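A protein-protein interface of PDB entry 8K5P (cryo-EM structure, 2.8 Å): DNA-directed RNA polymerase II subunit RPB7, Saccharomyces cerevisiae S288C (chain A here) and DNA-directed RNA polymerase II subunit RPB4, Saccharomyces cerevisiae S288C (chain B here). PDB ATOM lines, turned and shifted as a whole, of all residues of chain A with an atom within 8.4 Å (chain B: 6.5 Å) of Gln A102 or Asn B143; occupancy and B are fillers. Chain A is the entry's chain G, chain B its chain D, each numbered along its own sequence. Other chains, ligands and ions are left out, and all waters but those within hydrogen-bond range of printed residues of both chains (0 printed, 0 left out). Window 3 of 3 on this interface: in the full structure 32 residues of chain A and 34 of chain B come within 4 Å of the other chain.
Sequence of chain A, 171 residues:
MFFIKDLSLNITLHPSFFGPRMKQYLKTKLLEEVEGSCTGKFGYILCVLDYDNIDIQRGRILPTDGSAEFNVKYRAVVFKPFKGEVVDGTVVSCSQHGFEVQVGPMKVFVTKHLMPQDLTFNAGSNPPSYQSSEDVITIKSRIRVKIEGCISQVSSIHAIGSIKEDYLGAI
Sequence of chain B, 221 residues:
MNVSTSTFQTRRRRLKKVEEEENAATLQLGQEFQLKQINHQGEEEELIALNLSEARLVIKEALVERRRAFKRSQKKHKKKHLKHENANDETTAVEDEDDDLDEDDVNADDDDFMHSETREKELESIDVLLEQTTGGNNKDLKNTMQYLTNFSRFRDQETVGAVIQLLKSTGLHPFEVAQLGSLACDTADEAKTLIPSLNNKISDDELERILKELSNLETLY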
ATOM      1  N   LEU A  46     -31.264 -20.413  19.688  1.00  0.00           N
ATOM      2  CA  LEU A  46     -31.104 -21.733  19.086  1.00  0.00           C
ATOM      3  C   LEU A  46     -31.943 -22.779  19.810  1.00  0.00           C
ATOM      4  O   LEU A  46     -32.694 -23.532  19.178  1.00  0.00           O
ATOM      5  CB  LEU A  46     -29.628 -22.136  19.085  1.00  0.00           C
ATOM      6  CG  LEU A  46     -28.679 -21.368  18.162  1.00  0.00           C
ATOM      7  CD1 LEU A  46     -29.359 -21.026  16.842  1.00  0.00           C
ATOM      8  CD2 LEU A  46     -28.139 -20.115  18.839  1.00  0.00           C
ATOM      9  N   PHE A  79     -27.157 -16.468  19.899  1.00  0.00           N
ATOM     10  CA  PHE A  79     -26.084 -16.218  18.944  1.00  0.00           C
ATOM     11  C   PHE A  79     -26.230 -14.799  18.413  1.00  0.00           C
ATOM     12  O   PHE A  79     -27.283 -14.442  17.874  1.00  0.00           O
ATOM     13  CB  PHE A  79     -26.126 -17.233  17.799  1.00  0.00           C
ATOM     14  CG  PHE A  79     -25.152 -16.947  16.690  1.00  0.00           C
ATOM     15  CD1 PHE A  79     -23.869 -16.502  16.966  1.00  0.00           C
ATOM     16  CD2 PHE A  79     -25.519 -17.132  15.369  1.00  0.00           C
ATOM     17  CE1 PHE A  79     -22.976 -16.241  15.943  1.00  0.00           C
ATOM     18  CE2 PHE A  79     -24.630 -16.875  14.344  1.00  0.00           C
ATOM     19  CZ  PHE A  79     -23.357 -16.429  14.632  1.00  0.00           C
ATOM     20  N   VAL A  87     -13.827 -15.100  12.817  1.00  0.00           N
ATOM     21  CA  VAL A  87     -14.734 -16.235  12.940  1.00  0.00           C
ATOM     22  C   VAL A  87     -14.575 -17.096  11.695  1.00  0.00           C
ATOM     23  O   VAL A  87     -14.292 -16.593  10.606  1.00  0.00           O
ATOM     24  CB  VAL A  87     -16.197 -15.753  13.133  1.00  0.00           C
ATOM     25  CG1 VAL A  87     -16.550 -14.679  12.112  1.00  0.00           C
ATOM     26  CG2 VAL A  87     -17.177 -16.909  13.080  1.00  0.00           C
ATOM     27  N   ASP A  88     -14.760 -18.404  11.857  1.00  0.00           N
ATOM     28  CA  ASP A  88     -14.628 -19.369  10.775  1.00  0.00           C
ATOM     29  C   ASP A  88     -16.016 -19.688  10.233  1.00  0.00           C
ATOM     30  O   ASP A  88     -16.978 -19.813  10.995  1.00  0.00           O
ATOM     31  CB  ASP A  88     -13.930 -20.646  11.273  1.00  0.00           C
ATOM     32  CG  ASP A  88     -14.324 -21.899  10.491  1.00  0.00           C
ATOM     33  OD1 ASP A  88     -14.587 -21.820   9.271  1.00  0.00           O
ATOM     34  OD2 ASP A  88     -14.378 -22.982  11.112  1.00  0.00           O
ATOM     35  N   GLY A  89     -16.110 -19.815   8.908  1.00  0.00           N
ATOM     36  CA  GLY A  89     -17.372 -20.121   8.264  1.00  0.00           C
ATOM     37  C   GLY A  89     -17.161 -20.960   7.022  1.00  0.00           C
ATOM     38  O   GLY A  89     -16.032 -21.173   6.571  1.00  0.00           O
ATOM     39  N   THR A  90     -18.274 -21.436   6.470  1.00  0.00           N
ATOM     40  CA  THR A  90     -18.276 -22.278   5.282  1.00  0.00           C
ATOM     41  C   THR A  90     -19.140 -21.629   4.210  1.00  0.00           C
ATOM     42  O   THR A  90     -20.273 -21.223   4.484  1.00  0.00           O
ATOM     43  CB  THR A  90     -18.791 -23.685   5.606  1.00  0.00           C
ATOM     44  OG1 THR A  90     -17.766 -24.426   6.279  1.00  0.00           O
ATOM     45  CG2 THR A  90     -19.190 -24.422   4.337  1.00  0.00           C
ATOM     46  N   VAL A  91     -18.600 -21.532   2.993  1.00  0.00           N
ATOM     47  CA  VAL A  91     -19.329 -20.908   1.896  1.00  0.00           C
ATOM     48  C   VAL A  91     -20.530 -21.764   1.514  1.00  0.00           C
ATOM     49  O   VAL A  91     -20.501 -22.999   1.601  1.00  0.00           O
ATOM     50  CB  VAL A  91     -18.400 -20.688   0.687  1.00  0.00           C
ATOM     51  CG1 VAL A  91     -19.000 -19.672  -0.272  1.00  0.00           C
ATOM     52  CG2 VAL A  91     -17.022 -20.246   1.148  1.00  0.00           C
ATOM     53  N   VAL A  92     -21.611 -21.100   1.108  1.00  0.00           N
ATOM     54  CA  VAL A  92     -22.777 -21.791   0.561  1.00  0.00           C
ATOM     55  C   VAL A  92     -23.217 -21.243  -0.785  1.00  0.00           C
ATOM     56  O   VAL A  92     -23.998 -21.910  -1.489  1.00  0.00           O
ATOM     57  CB  VAL A  92     -23.957 -21.756   1.559  1.00  0.00           C
ATOM     58  CG1 VAL A  92     -23.579 -22.444   2.862  1.00  0.00           C
ATOM     59  CG2 VAL A  92     -24.403 -20.325   1.809  1.00  0.00           C
ATOM     60  N   SER A  93     -22.768 -20.060  -1.196  1.00  0.00           N
ATOM     61  CA  SER A  93     -23.144 -19.495  -2.482  1.00  0.00           C
ATOM     62  C   SER A  93     -22.020 -18.597  -2.974  1.00  0.00           C
ATOM     63  O   SER A  93     -21.201 -18.108  -2.191  1.00  0.00           O
ATOM     64  CB  SER A  93     -24.457 -18.710  -2.392  1.00  0.00           C
ATOM     65  OG  SER A  93     -24.632 -17.878  -3.526  1.00  0.00           O
ATOM     66  N   PHE A  99     -19.086 -13.950  -2.101  1.00  0.00           N
ATOM     67  CA  PHE A  99     -19.342 -15.302  -1.632  1.00  0.00           C
ATOM     68  C   PHE A  99     -20.167 -15.260  -0.352  1.00  0.00           C
ATOM     69  O   PHE A  99     -19.884 -14.472   0.556  1.00  0.00           O
ATOM     70  CB  PHE A  99     -18.035 -16.062  -1.392  1.00  0.00           C
ATOM     71  CG  PHE A  99     -16.883 -15.183  -0.997  1.00  0.00           C
ATOM     72  CD1 PHE A  99     -16.782 -14.686   0.291  1.00  0.00           C
ATOM     73  CD2 PHE A  99     -15.899 -14.856  -1.913  1.00  0.00           C
ATOM     74  CE1 PHE A  99     -15.724 -13.878   0.657  1.00  0.00           C
ATOM     75  CE2 PHE A  99     -14.837 -14.049  -1.555  1.00  0.00           C
ATOM     76  CZ  PHE A  99     -14.749 -13.559  -0.267  1.00  0.00           C
ATOM     77  N   GLU A 100     -21.192 -16.111  -0.291  1.00  0.00           N
ATOM     78  CA  GLU A 100     -22.099 -16.163   0.856  1.00  0.00           C
ATOM     79  C   GLU A 100     -21.529 -17.130   1.890  1.00  0.00           C
ATOM     80  O   GLU A 100     -21.889 -18.307   1.960  1.00  0.00           O
ATOM     81  CB  GLU A 100     -23.498 -16.572   0.414  1.00  0.00           C
ATOM     82  CG  GLU A 100     -24.436 -15.411   0.126  1.00  0.00           C
ATOM     83  CD  GLU A 100     -24.337 -14.307   1.160  1.00  0.00           C
ATOM     84  OE1 GLU A 100     -24.951 -14.444   2.239  1.00  0.00           O
ATOM     85  OE2 GLU A 100     -23.652 -13.300   0.892  1.00  0.00           O
ATOM     86  N   VAL A 101     -20.612 -16.612   2.708  1.00  0.00           N
ATOM     87  CA  VAL A 101     -20.058 -17.404   3.796  1.00  0.00           C
ATOM     88  C   VAL A 101     -21.128 -17.621   4.857  1.00  0.00           C
ATOM     89  O   VAL A 101     -21.846 -16.691   5.242  1.00  0.00           O
ATOM     90  CB  VAL A 101     -18.817 -16.717   4.390  1.00  0.00           C
ATOM     91  CG1 VAL A 101     -18.129 -17.639   5.385  1.00  0.00           C
ATOM     92  CG2 VAL A 101     -17.859 -16.307   3.284  1.00  0.00           C
ATOM     93  N   GLN A 102     -21.245 -18.860   5.329  1.00  0.00           N
ATOM     94  CA  GLN A 102     -22.241 -19.227   6.326  1.00  0.00           C
ATOM     95  C   GLN A 102     -21.536 -19.638   7.609  1.00  0.00           C
ATOM     96  O   GLN A 102     -20.724 -20.569   7.605  1.00  0.00           O
ATOM     97  CB  GLN A 102     -23.136 -20.361   5.821  1.00  0.00           C
ATOM     98  CG  GLN A 102     -23.948 -21.039   6.911  1.00  0.00           C
ATOM     99  CD  GLN A 102     -25.409 -21.190   6.540  1.00  0.00           C
ATOM    100  OE1 GLN A 102     -25.974 -20.347   5.844  1.00  0.00           O
ATOM    101  NE2 GLN A 102     -26.029 -22.268   7.005  1.00  0.00           N
ATOM    102  N   VAL A 103     -21.846 -18.944   8.700  1.00  0.00           N
ATOM    103  CA  VAL A 103     -21.365 -19.290  10.031  1.00  0.00           C
ATOM    104  C   VAL A 103     -22.582 -19.564  10.906  1.00  0.00           C
ATOM    105  O   VAL A 103     -23.367 -18.654  11.203  1.00  0.00           O
ATOM    106  CB  VAL A 103     -20.465 -18.197  10.625  1.00  0.00           C
ATOM    107  CG1 VAL A 103     -21.129 -16.824  10.555  1.00  0.00           C
ATOM    108  CG2 VAL A 103     -20.129 -18.533  12.064  1.00  0.00           C
ATOM    109  N   GLY A 104     -22.746 -20.819  11.316  1.00  0.00           N
ATOM    110  CA  GLY A 104     -23.911 -21.224  12.063  1.00  0.00           C
ATOM    111  C   GLY A 104     -25.184 -20.900  11.310  1.00  0.00           C
ATOM    112  O   GLY A 104     -25.326 -21.202  10.121  1.00  0.00           O
ATOM    113  N   PRO A 105     -26.144 -20.268  11.994  1.00  0.00           N
ATOM    114  CA  PRO A 105     -27.360 -19.774  11.338  1.00  0.00           C
ATOM    115  C   PRO A 105     -27.208 -18.350  10.803  1.00  0.00           C
ATOM    116  O   PRO A 105     -28.014 -17.463  11.099  1.00  0.00           O
ATOM    117  CB  PRO A 105     -28.400 -19.851  12.458  1.00  0.00           C
ATOM    118  CG  PRO A 105     -27.609 -19.615  13.708  1.00  0.00           C
ATOM    119  CD  PRO A 105     -26.192 -20.083  13.455  1.00  0.00           C
ATOM    120  N   MET A 106     -26.169 -18.123  10.002  1.00  0.00           N
ATOM    121  CA  MET A 106     -25.890 -16.803   9.454  1.00  0.00           C
ATOM    122  C   MET A 106     -25.446 -16.918   8.005  1.00  0.00           C
ATOM    123  O   MET A 106     -25.031 -17.981   7.537  1.00  0.00           O
ATOM    124  CB  MET A 106     -24.818 -16.059  10.263  1.00  0.00           C
ATOM    125  CG  MET A 106     -25.371 -15.199  11.377  1.00  0.00           C
ATOM    126  SD  MET A 106     -26.673 -14.119  10.762  1.00  0.00           S
ATOM    127  CE  MET A 106     -25.763 -12.591  10.551  1.00  0.00           C
ATOM    128  N   LYS A 107     -25.545 -15.791   7.298  1.00  0.00           N
ATOM    129  CA  LYS A 107     -25.091 -15.663   5.912  1.00  0.00           C
ATOM    130  C   LYS A 107     -24.459 -14.277   5.788  1.00  0.00           C
ATOM    131  O   LYS A 107     -25.150 -13.290   5.520  1.00  0.00           O
ATOM    132  CB  LYS A 107     -26.238 -15.856   4.929  1.00  0.00           C
ATOM    133  CG  LYS A 107     -26.624 -17.306   4.700  1.00  0.00           C
ATOM    134  CD  LYS A 107     -27.745 -17.423   3.681  1.00  0.00           C
ATOM    135  CE  LYS A 107     -28.179 -18.868   3.505  1.00  0.00           C
ATOM    136  NZ  LYS A 107     -29.311 -18.994   2.546  1.00  0.00           N
ATOM    137  N   VAL A 108     -23.147 -14.210   5.987  1.00  0.00           N
ATOM    138  CA  VAL A 108     -22.419 -12.948   5.943  1.00  0.00           C
ATOM    139  C   VAL A 108     -21.987 -12.680   4.507  1.00  0.00           C
ATOM    140  O   VAL A 108     -21.424 -13.555   3.840  1.00  0.00           O
ATOM    141  CB  VAL A 108     -21.213 -12.973   6.898  1.00  0.00           C
ATOM    142  CG1 VAL A 108     -20.419 -14.260   6.737  1.00  0.00           C
ATOM    143  CG2 VAL A 108     -20.326 -11.762   6.669  1.00  0.00           C
ATOM    144  N   PHE A 109     -22.264 -11.471   4.027  1.00  0.00           N
ATOM    145  CA  PHE A 109     -21.994 -11.089   2.649  1.00  0.00           C
ATOM    146  C   PHE A 109     -20.717 -10.263   2.567  1.00  0.00           C
ATOM    147  O   PHE A 109     -20.451  -9.421   3.429  1.00  0.00           O
ATOM    148  CB  PHE A 109     -23.166 -10.296   2.069  1.00  0.00           C
ATOM    149  CG  PHE A 109     -22.915  -9.758   0.689  1.00  0.00           C
ATOM    150  CD1 PHE A 109     -22.566 -10.607  -0.348  1.00  0.00           C
ATOM    151  CD2 PHE A 109     -23.030  -8.403   0.429  1.00  0.00           C
ATOM    152  CE1 PHE A 109     -22.337 -10.114  -1.618  1.00  0.00           C
ATOM    153  CE2 PHE A 109     -22.802  -7.904  -0.839  1.00  0.00           C
ATOM    154  CZ  PHE A 109     -22.454  -8.761  -1.863  1.00  0.00           C
ATOM    155  N   ILE A 139     -17.634 -23.341  -3.835  1.00  0.00           N
ATOM    156  CA  ILE A 139     -18.965 -23.413  -3.240  1.00  0.00           C
ATOM    157  C   ILE A 139     -18.891 -24.004  -1.837  1.00  0.00           C
ATOM    158  O   ILE A 139     -19.533 -23.507  -0.904  1.00  0.00           O
ATOM    159  CB  ILE A 139     -19.912 -24.219  -4.149  1.00  0.00           C
ATOM    160  CG1 ILE A 139     -20.286 -23.400  -5.387  1.00  0.00           C
ATOM    161  CG2 ILE A 139     -21.163 -24.646  -3.391  1.00  0.00           C
ATOM    162  CD1 ILE A 139     -20.849 -22.033  -5.067  1.00  0.00           C
ATOM    163  N   SER A 141     -15.987 -24.710   0.812  1.00  0.00           N
ATOM    164  CA  SER A 141     -14.579 -24.550   1.145  1.00  0.00           C
ATOM    165  C   SER A 141     -14.457 -23.899   2.515  1.00  0.00           C
ATOM    166  O   SER A 141     -15.415 -23.329   3.042  1.00  0.00           O
ATOM    167  CB  SER A 141     -13.842 -23.715   0.093  1.00  0.00           C
ATOM    168  OG  SER A 141     -12.471 -23.576   0.420  1.00  0.00           O
ATOM    169  N   ARG A 142     -13.257 -23.995   3.080  1.00  0.00           N
ATOM    170  CA  ARG A 142     -12.943 -23.372   4.356  1.00  0.00           C
ATOM    171  C   ARG A 142     -12.485 -21.936   4.135  1.00  0.00           C
ATOM    172  O   ARG A 142     -11.690 -21.659   3.232  1.00  0.00           O
ATOM    173  CB  ARG A 142     -11.856 -24.160   5.088  1.00  0.00           C
ATOM    174  CG  ARG A 142     -11.760 -23.852   6.571  1.00  0.00           C
ATOM    175  CD  ARG A 142     -12.909 -24.484   7.337  1.00  0.00           C
ATOM    176  NE  ARG A 142     -13.026 -25.913   7.069  1.00  0.00           N
ATOM    177  CZ  ARG A 142     -14.025 -26.473   6.400  1.00  0.00           C
ATOM    178  NH1 ARG A 142     -15.018 -25.749   5.909  1.00  0.00           N
ATOM    179  NH2 ARG A 142     -14.028 -27.789   6.218  1.00  0.00           N
ATOM    180  N   ILE A 143     -12.994 -21.027   4.960  1.00  0.00           N
ATOM    181  CA  ILE A 143     -12.654 -19.612   4.849  1.00  0.00           C
ATOM    182  C   ILE A 143     -12.796 -18.970   6.221  1.00  0.00           C
ATOM    183  O   ILE A 143     -13.757 -19.234   6.950  1.00  0.00           O
ATOM    184  CB  ILE A 143     -13.537 -18.905   3.796  1.00  0.00           C
ATOM    185  CG1 ILE A 143     -13.309 -17.392   3.823  1.00  0.00           C
ATOM    186  CG2 ILE A 143     -15.005 -19.233   4.019  1.00  0.00           C
ATOM    187  CD1 ILE A 143     -12.006 -16.960   3.190  1.00  0.00           C
ATOM    188  N   VAL A 145     -13.312 -15.425   8.105  1.00  0.00           N
ATOM    189  CA  VAL A 145     -13.903 -14.134   7.779  1.00  0.00           C
ATOM    190  C   VAL A 145     -13.874 -13.251   9.017  1.00  0.00           C
ATOM    191  O   VAL A 145     -14.219 -13.700  10.116  1.00  0.00           O
ATOM    192  CB  VAL A 145     -15.344 -14.289   7.256  1.00  0.00           C
ATOM    193  CG1 VAL A 145     -15.889 -12.948   6.797  1.00  0.00           C
ATOM    194  CG2 VAL A 145     -15.391 -15.301   6.123  1.00  0.00           C
ATOM    195  N   ASN B 138     -37.956 -24.842  13.084  1.00  0.00           N
ATOM    196  CA  ASN B 138     -36.595 -24.586  13.570  1.00  0.00           C
ATOM    197  C   ASN B 138     -35.535 -24.902  12.521  1.00  0.00           C
ATOM    198  O   ASN B 138     -34.644 -25.725  12.756  1.00  0.00           O
ATOM    199  CB  ASN B 138     -36.277 -25.315  14.894  1.00  0.00           C
ATOM    200  CG  ASN B 138     -36.549 -26.819  14.871  1.00  0.00           C
ATOM    201  OD1 ASN B 138     -37.497 -27.305  14.268  1.00  0.00           O
ATOM    202  ND2 ASN B 138     -35.690 -27.563  15.555  1.00  0.00           N
ATOM    203  N   LYS B 139     -35.629 -24.252  11.357  1.00  0.00           N
ATOM    204  CA  LYS B 139     -34.708 -24.546  10.264  1.00  0.00           C
ATOM    205  C   LYS B 139     -33.269 -24.221  10.646  1.00  0.00           C
ATOM    206  O   LYS B 139     -32.349 -24.980  10.323  1.00  0.00           O
ATOM    207  CB  LYS B 139     -35.122 -23.772   9.012  1.00  0.00           C
ATOM    208  CG  LYS B 139     -34.061 -23.726   7.924  1.00  0.00           C
ATOM    209  CD  LYS B 139     -33.830 -25.101   7.321  1.00  0.00           C
ATOM    210  CE  LYS B 139     -32.587 -25.117   6.452  1.00  0.00           C
ATOM    211  NZ  LYS B 139     -32.296 -26.475   5.920  1.00  0.00           N
ATOM    212  N   ASP B 140     -33.057 -23.104  11.343  1.00  0.00           N
ATOM    213  CA  ASP B 140     -31.704 -22.674  11.678  1.00  0.00           C
ATOM    214  C   ASP B 140     -30.974 -23.646  12.598  1.00  0.00           C
ATOM    215  O   ASP B 140     -29.742 -23.596  12.678  1.00  0.00           O
ATOM    216  CB  ASP B 140     -31.757 -21.251  12.264  1.00  0.00           C
ATOM    217  CG  ASP B 140     -32.162 -21.197  13.750  1.00  0.00           C
ATOM    218  OD1 ASP B 140     -32.627 -20.116  14.165  1.00  0.00           O
ATOM    219  OD2 ASP B 140     -32.041 -22.180  14.512  1.00  0.00           O
ATOM    220  N   LEU B 141     -31.701 -24.517  13.303  1.00  0.00           N
ATOM    221  CA  LEU B 141     -31.052 -25.448  14.220  1.00  0.00           C
ATOM    222  C   LEU B 141     -30.192 -26.464  13.480  1.00  0.00           C
ATOM    223  O   LEU B 141     -29.160 -26.899  14.006  1.00  0.00           O
ATOM    224  CB  LEU B 141     -32.096 -26.166  15.074  1.00  0.00           C
ATOM    225  CG  LEU B 141     -31.596 -26.814  16.368  1.00  0.00           C
ATOM    226  CD1 LEU B 141     -30.544 -25.949  17.047  1.00  0.00           C
ATOM    227  CD2 LEU B 141     -32.753 -27.090  17.312  1.00  0.00           C
ATOM    228  N   LYS B 142     -30.606 -26.872  12.279  1.00  0.00           N
ATOM    229  CA  LYS B 142     -29.814 -27.830  11.516  1.00  0.00           C
ATOM    230  C   LYS B 142     -28.470 -27.242  11.105  1.00  0.00           C
ATOM    231  O   LYS B 142     -27.436 -27.913  11.208  1.00  0.00           O
ATOM    232  CB  LYS B 142     -30.595 -28.298  10.289  1.00  0.00           C
ATOM    233  CG  LYS B 142     -32.024 -28.724  10.587  1.00  0.00           C
ATOM    234  CD  LYS B 142     -32.893 -28.651   9.344  1.00  0.00           C
ATOM    235  CE  LYS B 142     -34.352 -28.905   9.679  1.00  0.00           C
ATOM    236  NZ  LYS B 142     -35.242 -28.610   8.524  1.00  0.00           N
ATOM    237  N   ASN B 143     -28.461 -25.989  10.643  1.00  0.00           N
ATOM    238  CA  ASN B 143     -27.224 -25.383  10.160  1.00  0.00           C
ATOM    239  C   ASN B 143     -26.212 -25.210  11.286  1.00  0.00           C
ATOM    240  O   ASN B 143     -25.027 -25.527  11.123  1.00  0.00           O
ATOM    241  CB  ASN B 143     -27.526 -24.040   9.496  1.00  0.00           C
ATOM    242  CG  ASN B 143     -28.811 -24.063   8.695  1.00  0.00           C
ATOM    243  OD1 ASN B 143     -29.852 -24.498   9.186  1.00  0.00           O
ATOM    244  ND2 ASN B 143     -28.745 -23.591   7.457  1.00  0.00           N
ATOM    245  N   THR B 144     -26.658 -24.706  12.440  1.00  0.00           N
ATOM    246  CA  THR B 144     -25.734 -24.521  13.553  1.00  0.00           C
ATOM    247  C   THR B 144     -25.252 -25.855  14.107  1.00  0.00           C
ATOM    248  O   THR B 144     -24.092 -25.967  14.518  1.00  0.00           O
ATOM    249  CB  THR B 144     -26.381 -23.677  14.656  1.00  0.00           C
ATOM    250  OG1 THR B 144     -25.486 -23.581  15.772  1.00  0.00           O
ATOM    251  CG2 THR B 144     -27.692 -24.285  15.117  1.00  0.00           C
ATOM    252  N   MET B 145     -26.111 -26.877  14.116  1.00  0.00           N
ATOM    253  CA  MET B 145     -25.671 -28.199  14.549  1.00  0.00           C
ATOM    254  C   MET B 145     -24.627 -28.770  13.596  1.00  0.00           C
ATOM    255  O   MET B 145     -23.640 -29.370  14.036  1.00  0.00           O
ATOM    256  CB  MET B 145     -26.869 -29.143  14.668  1.00  0.00           C
ATOM    257  CG  MET B 145     -27.428 -29.366  16.087  1.00  0.00           C
ATOM    258  SD  MET B 145     -26.366 -29.365  17.563  1.00  0.00           S
ATOM    259  CE  MET B 145     -24.882 -30.237  17.049  1.00  0.00           C
ATOM    260  N   GLN B 146     -24.829 -28.591  12.288  1.00  0.00           N
ATOM    261  CA  GLN B 146     -23.833 -29.039  11.320  1.00  0.00           C
ATOM    262  C   GLN B 146     -22.516 -28.296  11.505  1.00  0.00           C
ATOM    263  O   GLN B 146     -21.436 -28.896  11.422  1.00  0.00           O
ATOM    264  CB  GLN B 146     -24.359 -28.852   9.898  1.00  0.00           C
ATOM    265  CG  GLN B 146     -25.434 -29.847   9.493  1.00  0.00           C
ATOM    266  CD  GLN B 146     -26.082 -29.495   8.168  1.00  0.00           C
ATOM    267  OE1 GLN B 146     -25.990 -28.359   7.703  1.00  0.00           O
ATOM    268  NE2 GLN B 146     -26.739 -30.470   7.553  1.00  0.00           N
ATOM    269  N   TYR B 147     -22.587 -26.986  11.755  1.00  0.00           N
ATOM    270  CA  TYR B 147     -21.376 -26.205  11.989  1.00  0.00           C
ATOM    271  C   TYR B 147     -20.653 -26.690  13.241  1.00  0.00           C
ATOM    272  O   TYR B 147     -19.421 -26.791  13.256  1.00  0.00           O
ATOM    273  CB  TYR B 147     -21.736 -24.713  12.069  1.00  0.00           C
ATOM    274  CG  TYR B 147     -20.636 -23.738  12.477  1.00  0.00           C
ATOM    275  CD1 TYR B 147     -20.018 -23.804  13.724  1.00  0.00           C
ATOM    276  CD2 TYR B 147     -20.208 -22.754  11.597  1.00  0.00           C
ATOM    277  CE1 TYR B 147     -19.023 -22.918  14.080  1.00  0.00           C
ATOM    278  CE2 TYR B 147     -19.211 -21.865  11.946  1.00  0.00           C
ATOM    279  CZ  TYR B 147     -18.623 -21.950  13.188  1.00  0.00           C
ATOM    280  OH  TYR B 147     -17.629 -21.065  13.540  1.00  0.00           O
ATOM    281  N   LEU B 148     -21.402 -26.991  14.302  1.00  0.00           N
ATOM    282  CA  LEU B 148     -20.781 -27.496  15.522  1.00  0.00           C
ATOM    283  C   LEU B 148     -20.145 -28.862  15.297  1.00  0.00           C
ATOM    284  O   LEU B 148     -19.064 -29.144  15.829  1.00  0.00           O
ATOM    285  CB  LEU B 148     -21.813 -27.563  16.648  1.00  0.00           C
ATOM    286  CG  LEU B 148     -22.277 -26.227  17.228  1.00  0.00           C
ATOM    287  CD1 LEU B 148     -23.698 -26.338  17.755  1.00  0.00           C
ATOM    288  CD2 LEU B 148     -21.332 -25.759  18.322  1.00  0.00           C
ATOM    289  N   PHE B 151     -16.971 -28.649  12.883  1.00  0.00           N
ATOM    290  CA  PHE B 151     -15.914 -27.789  13.404  1.00  0.00           C
ATOM    291  C   PHE B 151     -15.642 -28.052  14.881  1.00  0.00           C
ATOM    292  O   PHE B 151     -15.145 -27.167  15.584  1.00  0.00           O
ATOM    293  CB  PHE B 151     -16.261 -26.316  13.187  1.00  0.00           C
ATOM    294  CG  PHE B 151     -16.223 -25.890  11.748  1.00  0.00           C
ATOM    295  CD1 PHE B 151     -15.248 -26.374  10.894  1.00  0.00           C
ATOM    296  CD2 PHE B 151     -17.163 -25.003  11.251  1.00  0.00           C
ATOM    297  CE1 PHE B 151     -15.212 -25.983   9.570  1.00  0.00           C
ATOM    298  CE2 PHE B 151     -17.132 -24.608   9.927  1.00  0.00           C
ATOM    299  CZ  PHE B 151     -16.155 -25.099   9.086  1.00  0.00           C
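Among the printed residues, pairs that only touch across the chains: Leu A46 with Asp B140 (3.7 Å), Leu A46 with Leu B141 (3.9 Å), Asp A88 with Phe B151 (3.4 Å), Thr A90 with Phe B151 (3.3 Å), Val A103 with Tyr B147 (3.5 Å), Gly A104 with Asn B143 (3.6 Å), Gly A104 with Tyr B147 (3.2 Å), Pro A105 with Asp B140 (3.6 Å), Pro A105 with Thr B144 (3.8 Å) and Arg A142 with Phe B151 (3.3 Å).
Of the printed residues of chain B, Val A103 touches Tyr B147. Of the printed residues of chain B, Arg A142 touches Phe B151. Of the printed residues of chain A, Thr B144 touches Pro A105 (3.8 Å). The nearest residue of chain B that does not touch Gln A102 is Tyr B147 (4.6 Å).
OD1 of Asn B143 sits close to O of Lys B139 (2.8 Å). The backbone NH (N) of Gln A102 is in hydrogen-bond range of the backbone carbonyl oxygen (O) of Thr A90 (2.7 Å). The side-chain hydroxyl (OG1) of Thr A90 sits at hydrogen-bond distance from the guanidinium group (NH1) of Arg A142. NE2 of Gln A102 lies within hydrogen-bond range of O of Gly A104 (3.4 Å). The backbone carbonyl oxygen (O) of Met A106 sits close to the side-chain amide oxygen (OE1) of Gln A102, 3.1 Å away.
Along chain B the printed residues that touch a printed residue of chain A span positions 140 to 151. Of the 25 printed residues of chain A, 8 touch a printed residue of chain B. Hydrophobic or aromatic side chains of chain A within 4 Å of the printed part of chain B: Leu A46, Val A103 and Pro A105. Among the printed residues, no Asp or Glu carboxylate lies within 4 Å of a Lys or Arg side-chain nitrogen of the other chain.
The side-chain amide nitrogen of Asn B143 sits close to the side-chain amide nitrogen of Gln A102 (3.1 Å). O of Asp A88 lies within hydrogen-bond range of OH of Tyr B147.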
